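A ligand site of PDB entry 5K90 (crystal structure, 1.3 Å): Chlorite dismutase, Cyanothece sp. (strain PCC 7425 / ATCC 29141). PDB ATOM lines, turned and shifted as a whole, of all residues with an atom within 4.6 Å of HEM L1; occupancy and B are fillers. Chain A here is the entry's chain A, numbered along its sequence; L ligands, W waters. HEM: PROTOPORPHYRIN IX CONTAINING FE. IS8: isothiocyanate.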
ATOM      1  N   ASN A  64      10.878 -10.286  14.867  1.00  0.00           N
ATOM      2  CA  ASN A  64      11.342  -9.297  15.820  1.00  0.00           C
ATOM      3  C   ASN A  64      11.030  -9.668  17.256  1.00  0.00           C
ATOM      4  O   ASN A  64      10.136 -10.465  17.553  1.00  0.00           O
ATOM      5  CB  ASN A  64      10.687  -7.911  15.551  1.00  0.00           C
ATOM      6  CG  ASN A  64       9.182  -7.950  15.648  1.00  0.00           C
ATOM      7  OD1 ASN A  64       8.522  -8.474  14.738  1.00  0.00           O
ATOM      8  ND2 ASN A  64       8.631  -7.466  16.709  1.00  0.00           N
ATOM      9  N   ILE A  65      11.787  -9.005  18.155  1.00  0.00           N
ATOM     10  CA  ILE A  65      11.572  -9.067  19.583  1.00  0.00           C
ATOM     11  C   ILE A  65      10.191  -8.594  19.969  1.00  0.00           C
ATOM     12  O   ILE A  65       9.711  -7.521  19.521  1.00  0.00           O
ATOM     13  CB  ILE A  65      12.669  -8.257  20.303  1.00  0.00           C
ATOM     14  CG1 ILE A  65      14.025  -8.990  20.170  1.00  0.00           C
ATOM     15  CG2 ILE A  65      12.349  -8.028  21.730  1.00  0.00           C
ATOM     16  CD1 ILE A  65      14.135 -10.363  20.916  1.00  0.00           C
ATOM     17  N   ARG A  66       9.580  -9.334  20.895  1.00  0.00           N
ATOM     18  CA  ARG A  66       8.218  -9.117  21.374  1.00  0.00           C
ATOM     19  C   ARG A  66       8.135  -8.679  22.841  1.00  0.00           C
ATOM     20  O   ARG A  66       7.092  -8.158  23.247  1.00  0.00           O
ATOM     21  CB  ARG A  66       7.420 -10.449  21.211  1.00  0.00           C
ATOM     22  CG  ARG A  66       7.318 -11.057  19.842  1.00  0.00           C
ATOM     23  CD  ARG A  66       7.040 -10.062  18.706  1.00  0.00           C
ATOM     24  NE  ARG A  66       7.091 -10.667  17.414  1.00  0.00           N
ATOM     25  CZ  ARG A  66       6.108 -11.367  16.887  1.00  0.00           C
ATOM     26  NH1 ARG A  66       5.007 -11.576  17.587  1.00  0.00           N
ATOM     27  NH2 ARG A  66       6.267 -11.921  15.730  1.00  0.00           N
ATOM     28  N   TYR A  67       9.131  -8.994  23.685  1.00  0.00           N
ATOM     29  CA  TYR A  67       9.114  -8.728  25.132  1.00  0.00           C
ATOM     30  C   TYR A  67      10.418  -8.143  25.673  1.00  0.00           C
ATOM     31  O   TYR A  67      10.405  -7.381  26.644  1.00  0.00           O
ATOM     32  CB  TYR A  67       8.801 -10.075  25.891  1.00  0.00           C
ATOM     33  CG  TYR A  67       7.424 -10.628  25.583  1.00  0.00           C
ATOM     34  CD1 TYR A  67       6.288  -9.881  25.956  1.00  0.00           C
ATOM     35  CD2 TYR A  67       7.221 -11.796  24.818  1.00  0.00           C
ATOM     36  CE1 TYR A  67       5.027 -10.303  25.639  1.00  0.00           C
ATOM     37  CE2 TYR A  67       5.959 -12.274  24.512  1.00  0.00           C
ATOM     38  CZ  TYR A  67       4.844 -11.506  24.952  1.00  0.00           C
ATOM     39  OH  TYR A  67       3.549 -11.830  24.604  1.00  0.00           O
ATOM     40  N   ALA A  68      11.567  -8.605  25.198  1.00  0.00           N
ATOM     41  CA  ALA A  68      12.809  -8.204  25.845  1.00  0.00           C
ATOM     42  C   ALA A  68      13.046  -6.706  25.681  1.00  0.00           C
ATOM     43  O   ALA A  68      12.812  -6.137  24.611  1.00  0.00           O
ATOM     44  CB  ALA A  68      13.997  -8.989  25.291  1.00  0.00           C
ATOM     45  N   LEU A  76      21.936 -10.473  27.172  1.00  0.00           N
ATOM     46  CA  LEU A  76      21.922 -11.659  26.319  1.00  0.00           C
ATOM     47  C   LEU A  76      23.003 -11.576  25.251  1.00  0.00           C
ATOM     48  O   LEU A  76      23.723 -12.551  24.997  1.00  0.00           O
ATOM     49  CB  LEU A  76      20.555 -11.829  25.661  1.00  0.00           C
ATOM     50  CG  LEU A  76      19.346 -12.169  26.556  1.00  0.00           C
ATOM     51  CD1 LEU A  76      18.050 -11.873  25.880  1.00  0.00           C
ATOM     52  CD2 LEU A  76      19.419 -13.646  26.958  1.00  0.00           C
ATOM     53  N   ILE A  94      11.678 -27.989  20.539  1.00  0.00           N
ATOM     54  CA  ILE A  94      10.568 -27.963  21.496  1.00  0.00           C
ATOM     55  C   ILE A  94       9.452 -27.105  20.909  1.00  0.00           C
ATOM     56  O   ILE A  94       9.407 -25.865  21.151  1.00  0.00           O
ATOM     57  CB  ILE A  94      10.994 -27.508  22.903  1.00  0.00           C
ATOM     58  CG1 ILE A  94      12.148 -28.388  23.464  1.00  0.00           C
ATOM     59  CG2 ILE A  94       9.812 -27.642  23.858  1.00  0.00           C
ATOM     60  CD1 ILE A  94      12.632 -27.898  24.867  1.00  0.00           C
ATOM     61  N   ILE A  96       5.844 -25.561  21.003  1.00  0.00           N
ATOM     62  CA  ILE A  96       5.044 -25.115  22.123  1.00  0.00           C
ATOM     63  C   ILE A  96       3.787 -24.430  21.620  1.00  0.00           C
ATOM     64  O   ILE A  96       3.849 -23.636  20.678  1.00  0.00           O
ATOM     65  CB  ILE A  96       5.868 -24.166  23.018  1.00  0.00           C
ATOM     66  CG1 ILE A  96       6.959 -24.986  23.725  1.00  0.00           C
ATOM     67  CG2 ILE A  96       4.984 -23.342  23.989  1.00  0.00           C
ATOM     68  CD1 ILE A  96       8.006 -24.146  24.337  1.00  0.00           C
ATOM     69  N   LYS A  98       0.495 -22.064  23.214  1.00  0.00           N
ATOM     70  CA  LYS A  98      -0.087 -21.402  24.370  1.00  0.00           C
ATOM     71  C   LYS A  98      -1.608 -21.268  24.189  1.00  0.00           C
ATOM     72  O   LYS A  98      -2.142 -21.389  23.083  1.00  0.00           O
ATOM     73  CB  LYS A  98       0.584 -20.038  24.609  1.00  0.00           C
ATOM     74  CG  LYS A  98       2.107 -20.146  25.008  1.00  0.00           C
ATOM     75  CD  LYS A  98       2.661 -18.807  25.402  1.00  0.00           C
ATOM     76  CE  LYS A  98       4.068 -18.906  25.890  1.00  0.00           C
ATOM     77  NZ  LYS A  98       4.601 -17.708  26.523  1.00  0.00           N
ATOM     78  N   TRP A 102      -4.044 -16.831  26.972  1.00  0.00           N
ATOM     79  CA  TRP A 102      -2.793 -16.105  26.860  1.00  0.00           C
ATOM     80  C   TRP A 102      -2.872 -15.062  25.747  1.00  0.00           C
ATOM     81  O   TRP A 102      -2.546 -13.884  25.943  1.00  0.00           O
ATOM     82  CB  TRP A 102      -1.660 -17.087  26.559  1.00  0.00           C
ATOM     83  CG  TRP A 102      -0.366 -16.445  26.212  1.00  0.00           C
ATOM     84  CD1 TRP A 102       0.127 -16.224  24.931  1.00  0.00           C
ATOM     85  CD2 TRP A 102       0.581 -15.828  27.097  1.00  0.00           C
ATOM     86  NE1 TRP A 102       1.338 -15.601  24.990  1.00  0.00           N
ATOM     87  CE2 TRP A 102       1.639 -15.339  26.303  1.00  0.00           C
ATOM     88  CE3 TRP A 102       0.646 -15.681  28.478  1.00  0.00           C
ATOM     89  CZ2 TRP A 102       2.731 -14.684  26.859  1.00  0.00           C
ATOM     90  CZ3 TRP A 102       1.743 -15.042  29.032  1.00  0.00           C
ATOM     91  CH2 TRP A 102       2.765 -14.518  28.208  1.00  0.00           C
ATOM     92  N   PHE A 114       5.561 -12.894  31.590  1.00  0.00           N
ATOM     93  CA  PHE A 114       6.732 -13.468  30.956  1.00  0.00           C
ATOM     94  C   PHE A 114       7.987 -13.175  31.761  1.00  0.00           C
ATOM     95  O   PHE A 114       8.803 -14.092  32.002  1.00  0.00           O
ATOM     96  CB  PHE A 114       6.846 -12.938  29.525  1.00  0.00           C
ATOM     97  CG  PHE A 114       8.071 -13.434  28.793  1.00  0.00           C
ATOM     98  CD1 PHE A 114       8.107 -14.682  28.195  1.00  0.00           C
ATOM     99  CD2 PHE A 114       9.170 -12.579  28.654  1.00  0.00           C
ATOM    100  CE1 PHE A 114       9.246 -15.080  27.494  1.00  0.00           C
ATOM    101  CE2 PHE A 114      10.266 -12.957  27.933  1.00  0.00           C
ATOM    102  CZ  PHE A 114      10.311 -14.242  27.403  1.00  0.00           C
ATOM    103  N   HIS A 120      11.663 -15.253  32.709  1.00  0.00           N
ATOM    104  CA  HIS A 120      12.078 -16.106  31.614  1.00  0.00           C
ATOM    105  C   HIS A 120      13.492 -15.783  31.156  1.00  0.00           C
ATOM    106  O   HIS A 120      14.342 -16.690  31.082  1.00  0.00           O
ATOM    107  CB  HIS A 120      11.076 -15.969  30.467  1.00  0.00           C
ATOM    108  CG  HIS A 120      11.309 -16.917  29.330  1.00  0.00           C
ATOM    109  ND1 HIS A 120      10.377 -17.858  28.943  1.00  0.00           N
ATOM    110  CD2 HIS A 120      12.372 -17.078  28.505  1.00  0.00           C
ATOM    111  CE1 HIS A 120      10.833 -18.530  27.898  1.00  0.00           C
ATOM    112  NE2 HIS A 120      12.058 -18.095  27.637  1.00  0.00           N
ATOM    113  N   THR A 121      13.805 -14.516  30.889  1.00  0.00           N
ATOM    114  CA  THR A 121      15.148 -14.145  30.455  1.00  0.00           C
ATOM    115  C   THR A 121      16.188 -14.303  31.576  1.00  0.00           C
ATOM    116  O   THR A 121      17.289 -14.832  31.356  1.00  0.00           O
ATOM    117  CB  THR A 121      15.117 -12.721  29.904  1.00  0.00           C
ATOM    118  OG1 THR A 121      14.358 -12.756  28.709  1.00  0.00           O
ATOM    119  CG2 THR A 121      16.497 -12.205  29.602  1.00  0.00           C
ATOM    120  N   GLY A 124      16.828 -18.007  32.048  1.00  0.00           N
ATOM    121  CA  GLY A 124      17.529 -18.505  30.876  1.00  0.00           C
ATOM    122  C   GLY A 124      18.972 -18.077  30.820  1.00  0.00           C
ATOM    123  O   GLY A 124      19.859 -18.886  30.508  1.00  0.00           O
ATOM    124  N   LEU A 125      19.260 -16.841  31.218  1.00  0.00           N
ATOM    125  CA  LEU A 125      20.634 -16.349  31.212  1.00  0.00           C
ATOM    126  C   LEU A 125      21.569 -17.175  32.113  1.00  0.00           C
ATOM    127  O   LEU A 125      22.793 -17.173  31.913  1.00  0.00           O
ATOM    128  CB  LEU A 125      20.667 -14.894  31.644  1.00  0.00           C
ATOM    129  CG  LEU A 125      20.491 -13.844  30.549  1.00  0.00           C
ATOM    130  CD1 LEU A 125      20.100 -12.527  31.174  1.00  0.00           C
ATOM    131  CD2 LEU A 125      21.822 -13.735  29.781  1.00  0.00           C
ATOM    132  N   LEU A 128      23.514 -19.639  29.909  1.00  0.00           N
ATOM    133  CA  LEU A 128      24.441 -19.202  28.902  1.00  0.00           C
ATOM    134  C   LEU A 128      25.815 -19.022  29.540  1.00  0.00           C
ATOM    135  O   LEU A 128      25.920 -18.595  30.691  1.00  0.00           O
ATOM    136  CB  LEU A 128      23.964 -17.851  28.332  1.00  0.00           C
ATOM    137  CG  LEU A 128      22.848 -18.004  27.289  1.00  0.00           C
ATOM    138  CD1 LEU A 128      21.767 -18.987  27.657  1.00  0.00           C
ATOM    139  CD2 LEU A 128      22.269 -16.611  27.044  1.00  0.00           C
ATOM    140  N   VAL A 131      24.220 -23.016  26.547  1.00  0.00           N
ATOM    141  CA  VAL A 131      23.091 -23.292  25.661  1.00  0.00           C
ATOM    142  C   VAL A 131      22.924 -22.169  24.626  1.00  0.00           C
ATOM    143  O   VAL A 131      22.748 -20.998  25.003  1.00  0.00           O
ATOM    144  CB  VAL A 131      21.804 -23.468  26.476  1.00  0.00           C
ATOM    145  CG1 VAL A 131      20.614 -23.654  25.566  1.00  0.00           C
ATOM    146  CG2 VAL A 131      21.962 -24.658  27.460  1.00  0.00           C
ATOM    147  N   ARG A 133      20.436 -20.896  21.296  1.00  0.00           N
ATOM    148  CA  ARG A 133      19.009 -21.078  21.051  1.00  0.00           C
ATOM    149  C   ARG A 133      18.576 -20.336  19.789  1.00  0.00           C
ATOM    150  O   ARG A 133      19.266 -19.428  19.317  1.00  0.00           O
ATOM    151  CB  ARG A 133      18.163 -20.562  22.226  1.00  0.00           C
ATOM    152  CG  ARG A 133      18.082 -19.029  22.282  1.00  0.00           C
ATOM    153  CD  ARG A 133      17.618 -18.539  23.672  1.00  0.00           C
ATOM    154  NE  ARG A 133      17.400 -17.097  23.608  1.00  0.00           N
ATOM    155  CZ  ARG A 133      18.376 -16.188  23.740  1.00  0.00           C
ATOM    156  NH1 ARG A 133      19.655 -16.517  23.957  1.00  0.00           N
ATOM    157  NH2 ARG A 133      18.065 -14.913  23.646  1.00  0.00           N
ATOM    158  N   LEU A 135      14.558 -18.892  18.307  1.00  0.00           N
ATOM    159  CA  LEU A 135      13.132 -18.800  18.505  1.00  0.00           C
ATOM    160  C   LEU A 135      12.464 -18.593  17.156  1.00  0.00           C
ATOM    161  O   LEU A 135      12.827 -17.668  16.435  1.00  0.00           O
ATOM    162  CB  LEU A 135      12.782 -17.702  19.494  1.00  0.00           C
ATOM    163  CG  LEU A 135      11.271 -17.376  19.617  1.00  0.00           C
ATOM    164  CD1 LEU A 135      10.566 -18.578  20.257  1.00  0.00           C
ATOM    165  CD2 LEU A 135      11.091 -16.157  20.481  1.00  0.00           C
ATOM    166  N   PHE A 147       5.019 -21.865  18.585  1.00  0.00           N
ATOM    167  CA  PHE A 147       6.423 -21.536  18.546  1.00  0.00           C
ATOM    168  C   PHE A 147       7.196 -22.797  18.283  1.00  0.00           C
ATOM    169  O   PHE A 147       6.782 -23.879  18.705  1.00  0.00           O
ATOM    170  CB  PHE A 147       6.987 -20.954  19.852  1.00  0.00           C
ATOM    171  CG  PHE A 147       6.204 -19.789  20.395  1.00  0.00           C
ATOM    172  CD1 PHE A 147       6.482 -18.494  19.987  1.00  0.00           C
ATOM    173  CD2 PHE A 147       5.215 -19.978  21.365  1.00  0.00           C
ATOM    174  CE1 PHE A 147       5.735 -17.451  20.484  1.00  0.00           C
ATOM    175  CE2 PHE A 147       4.488 -18.939  21.851  1.00  0.00           C
ATOM    176  CZ  PHE A 147       4.769 -17.647  21.421  1.00  0.00           C
ATOM    177  N   THR A 149      10.876 -23.804  19.347  1.00  0.00           N
ATOM    178  CA  THR A 149      12.064 -23.405  20.070  1.00  0.00           C
ATOM    179  C   THR A 149      13.148 -24.452  19.789  1.00  0.00           C
ATOM    180  O   THR A 149      12.842 -25.610  19.579  1.00  0.00           O
ATOM    181  CB  THR A 149      11.775 -23.131  21.550  1.00  0.00           C
ATOM    182  OG1 THR A 149      11.469 -24.340  22.249  1.00  0.00           O
ATOM    183  CG2 THR A 149      10.614 -22.221  21.780  1.00  0.00           C
ATOM    184  N   PHE A 151      17.272 -25.459  20.916  1.00  0.00           N
ATOM    185  CA  PHE A 151      18.397 -25.307  21.806  1.00  0.00           C
ATOM    186  C   PHE A 151      19.498 -26.253  21.358  1.00  0.00           C
ATOM    187  O   PHE A 151      19.242 -27.395  20.911  1.00  0.00           O
ATOM    188  CB  PHE A 151      17.990 -25.610  23.258  1.00  0.00           C
ATOM    189  CG  PHE A 151      16.810 -24.771  23.662  1.00  0.00           C
ATOM    190  CD1 PHE A 151      17.001 -23.448  24.065  1.00  0.00           C
ATOM    191  CD2 PHE A 151      15.543 -25.248  23.473  1.00  0.00           C
ATOM    192  CE1 PHE A 151      15.889 -22.629  24.310  1.00  0.00           C
ATOM    193  CE2 PHE A 151      14.410 -24.419  23.737  1.00  0.00           C
ATOM    194  CZ  PHE A 151      14.603 -23.115  24.152  1.00  0.00           C
ATOM    195  N   PHE A 161      20.573 -28.387  31.174  1.00  0.00           N
ATOM    196  CA  PHE A 161      19.424 -28.079  30.326  1.00  0.00           C
ATOM    197  C   PHE A 161      18.151 -28.774  30.843  1.00  0.00           C
ATOM    198  O   PHE A 161      17.087 -28.181  30.891  1.00  0.00           O
ATOM    199  CB  PHE A 161      19.688 -28.409  28.859  1.00  0.00           C
ATOM    200  CG  PHE A 161      18.562 -27.986  27.927  1.00  0.00           C
ATOM    201  CD1 PHE A 161      18.406 -26.654  27.561  1.00  0.00           C
ATOM    202  CD2 PHE A 161      17.648 -28.919  27.428  1.00  0.00           C
ATOM    203  CE1 PHE A 161      17.372 -26.252  26.762  1.00  0.00           C
ATOM    204  CE2 PHE A 161      16.580 -28.479  26.586  1.00  0.00           C
ATOM    205  CZ  PHE A 161      16.482 -27.157  26.244  1.00  0.00           C
ATOM    206  N   LEU A 164      16.908 -26.619  33.610  1.00  0.00           N
ATOM    207  CA  LEU A 164      16.233 -25.438  33.069  1.00  0.00           C
ATOM    208  C   LEU A 164      14.813 -25.776  32.647  1.00  0.00           C
ATOM    209  O   LEU A 164      13.876 -25.000  32.913  1.00  0.00           O
ATOM    210  CB  LEU A 164      17.086 -24.906  31.917  1.00  0.00           C
ATOM    211  CG  LEU A 164      16.345 -23.820  31.122  1.00  0.00           C
ATOM    212  CD1 LEU A 164      16.112 -22.560  31.932  1.00  0.00           C
ATOM    213  CD2 LEU A 164      17.156 -23.589  29.910  1.00  0.00           C
ATOM    214  N   LEU A 165      14.625 -26.882  31.949  1.00  0.00           N
ATOM    215  CA  LEU A 165      13.272 -27.248  31.514  1.00  0.00           C
ATOM    216  C   LEU A 165      12.332 -27.343  32.704  1.00  0.00           C
ATOM    217  O   LEU A 165      11.175 -26.920  32.641  1.00  0.00           O
ATOM    218  CB  LEU A 165      13.294 -28.584  30.770  1.00  0.00           C
ATOM    219  CG  LEU A 165      13.863 -28.612  29.339  1.00  0.00           C
ATOM    220  CD1 LEU A 165      13.826 -30.035  28.794  1.00  0.00           C
ATOM    221  CD2 LEU A 165      13.169 -27.664  28.365  1.00  0.00           C
ATOM    222  N   MET A 168      11.425 -23.868  34.058  1.00  0.00           N
ATOM    223  CA  MET A 168      10.453 -23.146  33.224  1.00  0.00           C
ATOM    224  C   MET A 168       9.049 -23.704  33.424  1.00  0.00           C
ATOM    225  O   MET A 168       8.094 -22.951  33.601  1.00  0.00           O
ATOM    226  CB  MET A 168      10.864 -23.230  31.771  1.00  0.00           C
ATOM    227  CG  MET A 168      12.330 -23.030  31.616  1.00  0.00           C
ATOM    228  SD  MET A 168      12.873 -22.056  30.251  1.00  0.00           S
ATOM    229  CE  MET A 168      12.837 -20.383  30.932  1.00  0.00           C
ATOM    230  N   GLU A 173       4.270 -18.450  33.561  1.00  0.00           N
ATOM    231  CA  GLU A 173       4.126 -18.489  32.111  1.00  0.00           C
ATOM    232  C   GLU A 173       3.689 -19.861  31.633  1.00  0.00           C
ATOM    233  O   GLU A 173       2.894 -19.989  30.684  1.00  0.00           O
ATOM    234  CB  GLU A 173       5.428 -18.088  31.417  1.00  0.00           C
ATOM    235  CG  GLU A 173       5.427 -18.343  29.896  1.00  0.00           C
ATOM    236  CD  GLU A 173       6.757 -18.056  29.244  1.00  0.00           C
ATOM    237  OE1 GLU A 173       7.807 -18.001  29.930  1.00  0.00           O
ATOM    238  OE2 GLU A 173       6.784 -17.881  28.011  1.00  0.00           O
ATOM    239  N   TRP A 174       4.223 -20.934  32.240  1.00  0.00           N
ATOM    240  CA  TRP A 174       3.885 -22.272  31.766  1.00  0.00           C
ATOM    241  C   TRP A 174       2.466 -22.707  32.106  1.00  0.00           C
ATOM    242  O   TRP A 174       1.998 -23.708  31.547  1.00  0.00           O
ATOM    243  CB  TRP A 174       4.919 -23.318  32.263  1.00  0.00           C
ATOM    244  CG  TRP A 174       5.603 -23.909  31.112  1.00  0.00           C
ATOM    245  CD1 TRP A 174       5.438 -25.173  30.602  1.00  0.00           C
ATOM    246  CD2 TRP A 174       6.576 -23.276  30.322  1.00  0.00           C
ATOM    247  NE1 TRP A 174       6.239 -25.346  29.528  1.00  0.00           N
ATOM    248  CE2 TRP A 174       6.936 -24.186  29.313  1.00  0.00           C
ATOM    249  CE3 TRP A 174       7.146 -22.006  30.322  1.00  0.00           C
ATOM    250  CZ2 TRP A 174       7.871 -23.885  28.339  1.00  0.00           C
ATOM    251  CZ3 TRP A 174       8.050 -21.702  29.350  1.00  0.00           C
ATOM    252  CH2 TRP A 174       8.428 -22.636  28.377  1.00  0.00           C
ATOM    253  N   GLU A 180       3.101 -29.332  24.229  1.00  0.00           N
ATOM    254  CA  GLU A 180       4.550 -29.220  24.281  1.00  0.00           C
ATOM    255  C   GLU A 180       5.133 -30.598  23.978  1.00  0.00           C
ATOM    256  O   GLU A 180       4.676 -31.605  24.523  1.00  0.00           O
ATOM    257  CB  GLU A 180       4.949 -28.703  25.665  1.00  0.00           C
ATOM    258  CG  GLU A 180       6.447 -28.512  25.817  1.00  0.00           C
ATOM    259  CD  GLU A 180       6.888 -27.933  27.148  1.00  0.00           C
ATOM    260  OE1 GLU A 180       6.070 -27.775  28.067  1.00  0.00           O
ATOM    261  OE2 GLU A 180       8.111 -27.674  27.285  1.00  0.00           O
HETATM  262  CHA HEM L   1      10.903 -16.520  24.233  1.00  0.00           C
HETATM  263  CHB HEM L   1      15.262 -16.406  26.313  1.00  0.00           C
HETATM  264  CHC HEM L   1      15.062 -21.053  27.234  1.00  0.00           C
HETATM  265  CHD HEM L   1      10.584 -21.181  25.362  1.00  0.00           C
HETATM  266  C1A HEM L   1      12.085 -16.044  24.735  1.00  0.00           C
HETATM  267  C2A HEM L   1      12.567 -14.679  24.780  1.00  0.00           C
HETATM  268  C3A HEM L   1      13.763 -14.646  25.360  1.00  0.00           C
HETATM  269  C4A HEM L   1      14.083 -16.011  25.695  1.00  0.00           C
HETATM  270  CMA HEM L   1      14.678 -13.439  25.670  1.00  0.00           C
HETATM  271  CAA HEM L   1      11.777 -13.468  24.301  1.00  0.00           C
HETATM  272  CBA HEM L   1      12.138 -13.094  22.905  1.00  0.00           C
HETATM  273  CGA HEM L   1      11.237 -11.886  22.520  1.00  0.00           C
HETATM  274  O1A HEM L   1      10.493 -11.925  21.526  1.00  0.00           O
HETATM  275  O2A HEM L   1      11.229 -10.876  23.283  1.00  0.00           O
HETATM  276  C1B HEM L   1      15.620 -17.682  26.696  1.00  0.00           C
HETATM  277  C2B HEM L   1      16.930 -18.043  27.163  1.00  0.00           C
HETATM  278  C3B HEM L   1      16.897 -19.351  27.393  1.00  0.00           C
HETATM  279  C4B HEM L   1      15.579 -19.803  27.088  1.00  0.00           C
HETATM  280  CMB HEM L   1      18.144 -17.084  27.348  1.00  0.00           C
HETATM  281  CAB HEM L   1      18.036 -20.242  27.867  1.00  0.00           C
HETATM  282  CBB HEM L   1      18.232 -21.438  27.269  1.00  0.00           C
HETATM  283  C1C HEM L   1      13.858 -21.516  26.855  1.00  0.00           C
HETATM  284  C2C HEM L   1      13.332 -22.839  26.941  1.00  0.00           C
HETATM  285  C3C HEM L   1      12.126 -22.880  26.402  1.00  0.00           C
HETATM  286  C4C HEM L   1      11.772 -21.534  25.953  1.00  0.00           C
HETATM  287  CMC HEM L   1      14.135 -23.999  27.470  1.00  0.00           C
HETATM  288  CAC HEM L   1      11.177 -24.078  26.219  1.00  0.00           C
HETATM  289  CBC HEM L   1      11.071 -25.026  27.128  1.00  0.00           C
HETATM  290  C1D HEM L   1      10.347 -19.944  24.849  1.00  0.00           C
HETATM  291  C2D HEM L   1       9.088 -19.555  24.243  1.00  0.00           C
HETATM  292  C3D HEM L   1       9.201 -18.313  23.871  1.00  0.00           C
HETATM  293  C4D HEM L   1      10.426 -17.782  24.371  1.00  0.00           C
HETATM  294  CMD HEM L   1       7.930 -20.452  23.899  1.00  0.00           C
HETATM  295  CAD HEM L   1       8.164 -17.361  23.209  1.00  0.00           C
HETATM  296  CBD HEM L   1       7.461 -16.531  24.299  1.00  0.00           C
HETATM  297  CGD HEM L   1       6.239 -15.761  23.775  1.00  0.00           C
HETATM  298  O1D HEM L   1       6.345 -14.983  22.781  1.00  0.00           O
HETATM  299  O2D HEM L   1       5.112 -15.912  24.349  1.00  0.00           O
HETATM  300  NA  HEM L   1      13.055 -16.838  25.296  1.00  0.00           N
HETATM  301  NB  HEM L   1      14.827 -18.774  26.610  1.00  0.00           N
HETATM  302  NC  HEM L   1      12.862 -20.730  26.301  1.00  0.00           N
HETATM  303  ND  HEM L   1      11.138 -18.819  24.963  1.00  0.00           N
HETATM  304 FE   HEM L   1      12.998 -18.724  25.841  1.00  0.00          FE
HETATM  305  S   IS8 L   2      14.356 -20.336  21.505  1.00  0.00           S
HETATM  306  C   IS8 L   2      13.967 -19.730  22.911  1.00  0.00           C
HETATM  307  N   IS8 L   2      13.768 -19.300  24.006  1.00  0.00           N
HETATM  308  O   HOH W   1       3.331 -14.202  23.430  1.00  0.00           O
HETATM  309  O   HOH W   2       4.621 -13.732  20.938  1.00  0.00           O
HETATM  310  O   HOH W   3      14.925 -16.674  22.512  1.00  0.00           O
HETATM  311  O   HOH W   4       8.465 -14.005  21.415  1.00  0.00           O
HETATM  312  O   HOH W   5      10.835 -12.772  18.981  1.00  0.00           O
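Ile 65 touches HEM L1 (CG2 to O2A, 3.4 Å).
Leu 76 touches HEM L1.
Ile 94 touches HEM L1 (CD1 to CBC, 3.97 Å).
Ile 96 touches HEM L1 (CD1 to CAC, 3.7 Å).
Trp 102 touches HEM L1.
Phe 114 touches HEM L1.
Thr 121 touches HEM L1 (OG1 to CMA, 3.1 Å).
O of Gly 124 touches CAB of HEM L1, 3.5 Å away.
Leu 128 touches HEM L1.
Val 131 touches HEM L1.
NE of Arg 133 touches CHB of HEM L1, 3.5 Å away.
CD2 of Leu 135 touches CHA of HEM L1, at 3.8 Å.
Phe 147 touches HEM L1.
CG2 of Thr 149 touches CHD of HEM L1, 3.7 Å away.
Phe 151 touches HEM L1.
Leu 164 touches HEM L1 (CD2 to CBB, 3.6 Å).
CD2 of Leu 165 touches CBC of HEM L1, 3.6 Å away.
Met 168 touches HEM L1.
Trp 174 touches HEM L1.
Glu 180 touches HEM L1.
25 residues have an atom within 4 Å of HEM L1: Ile 65, Arg 66, Tyr 67, Ala 68, Leu 76, Ile 94, Ile 96, Lys 98, Trp 102, Phe 114, His 120, Thr 121, Gly 124, Leu 128, Val 131, Arg 133, Leu 135, Phe 147, Thr 149, Phe 151, Leu 164, Leu 165, Met 168, Trp 174 and Glu 180.
The nearest printed residue that does not touch HEM L1 is Phe 161 (4.01 Å).
An iron atom (FE) of HEM L1 is bound by a nitrogen (N) of IS8 L2 (2.1 Å).
The backbone NH (N) of His 120 lies within hydrogen-bond range of the backbone carbonyl oxygen (O) of Phe 114.
OE1 of Glu 173 sits at hydrogen-bond distance from ND1 of His 120.
The guanidinium group (NE) of Arg 66 lies within hydrogen-bond range of the backbone carbonyl oxygen (O) of Asn 64 (3.1 Å).
The side-chain carboxylate (OE2) of Glu 173 lies within salt-bridge range of the side-chain amino group (NZ) of Lys 98 (2.6 Å).
The backbone carbonyl oxygen (O) of Ile 96 is in hydrogen-bond range of the backbone NH (N) of Phe 147.
OE1 of Glu 180 lies within hydrogen-bond range of NE1 of Trp 174 (2.8 Å).
The side-chain hydroxyl of Thr 149 lies within hydrogen-bond range of the backbone carbonyl oxygen of Ile 94, 2.8 Å away.
Water W1 lies within hydrogen-bond range of O2D of HEM L1, OH of Tyr 67 and NE1 of Trp 102.
Water W5 bridges an oxygen (O1A) of HEM L1 (2.7 Å) and the backbone carbonyl oxygen of Asn 64 (2.8 Å).
FE of HEM L1 is bound by NE2 of His 120 (2.1 Å).
The backbone NH of Arg 66 lies within hydrogen-bond range of an oxygen (O1A) of HEM L1 (2.8 Å).
N of Tyr 67 lies within hydrogen-bond range of O2A of HEM L1, 2.8 Å away.
NZ of Lys 98 is in salt-bridge range of O2D of HEM L1, 2.9 Å away.
O2A of HEM L1 sits at hydrogen-bond distance from N of Ala 68, 3.0 Å away.
S of IS8 L2 sits close to N of Leu 135 (3.5 Å).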
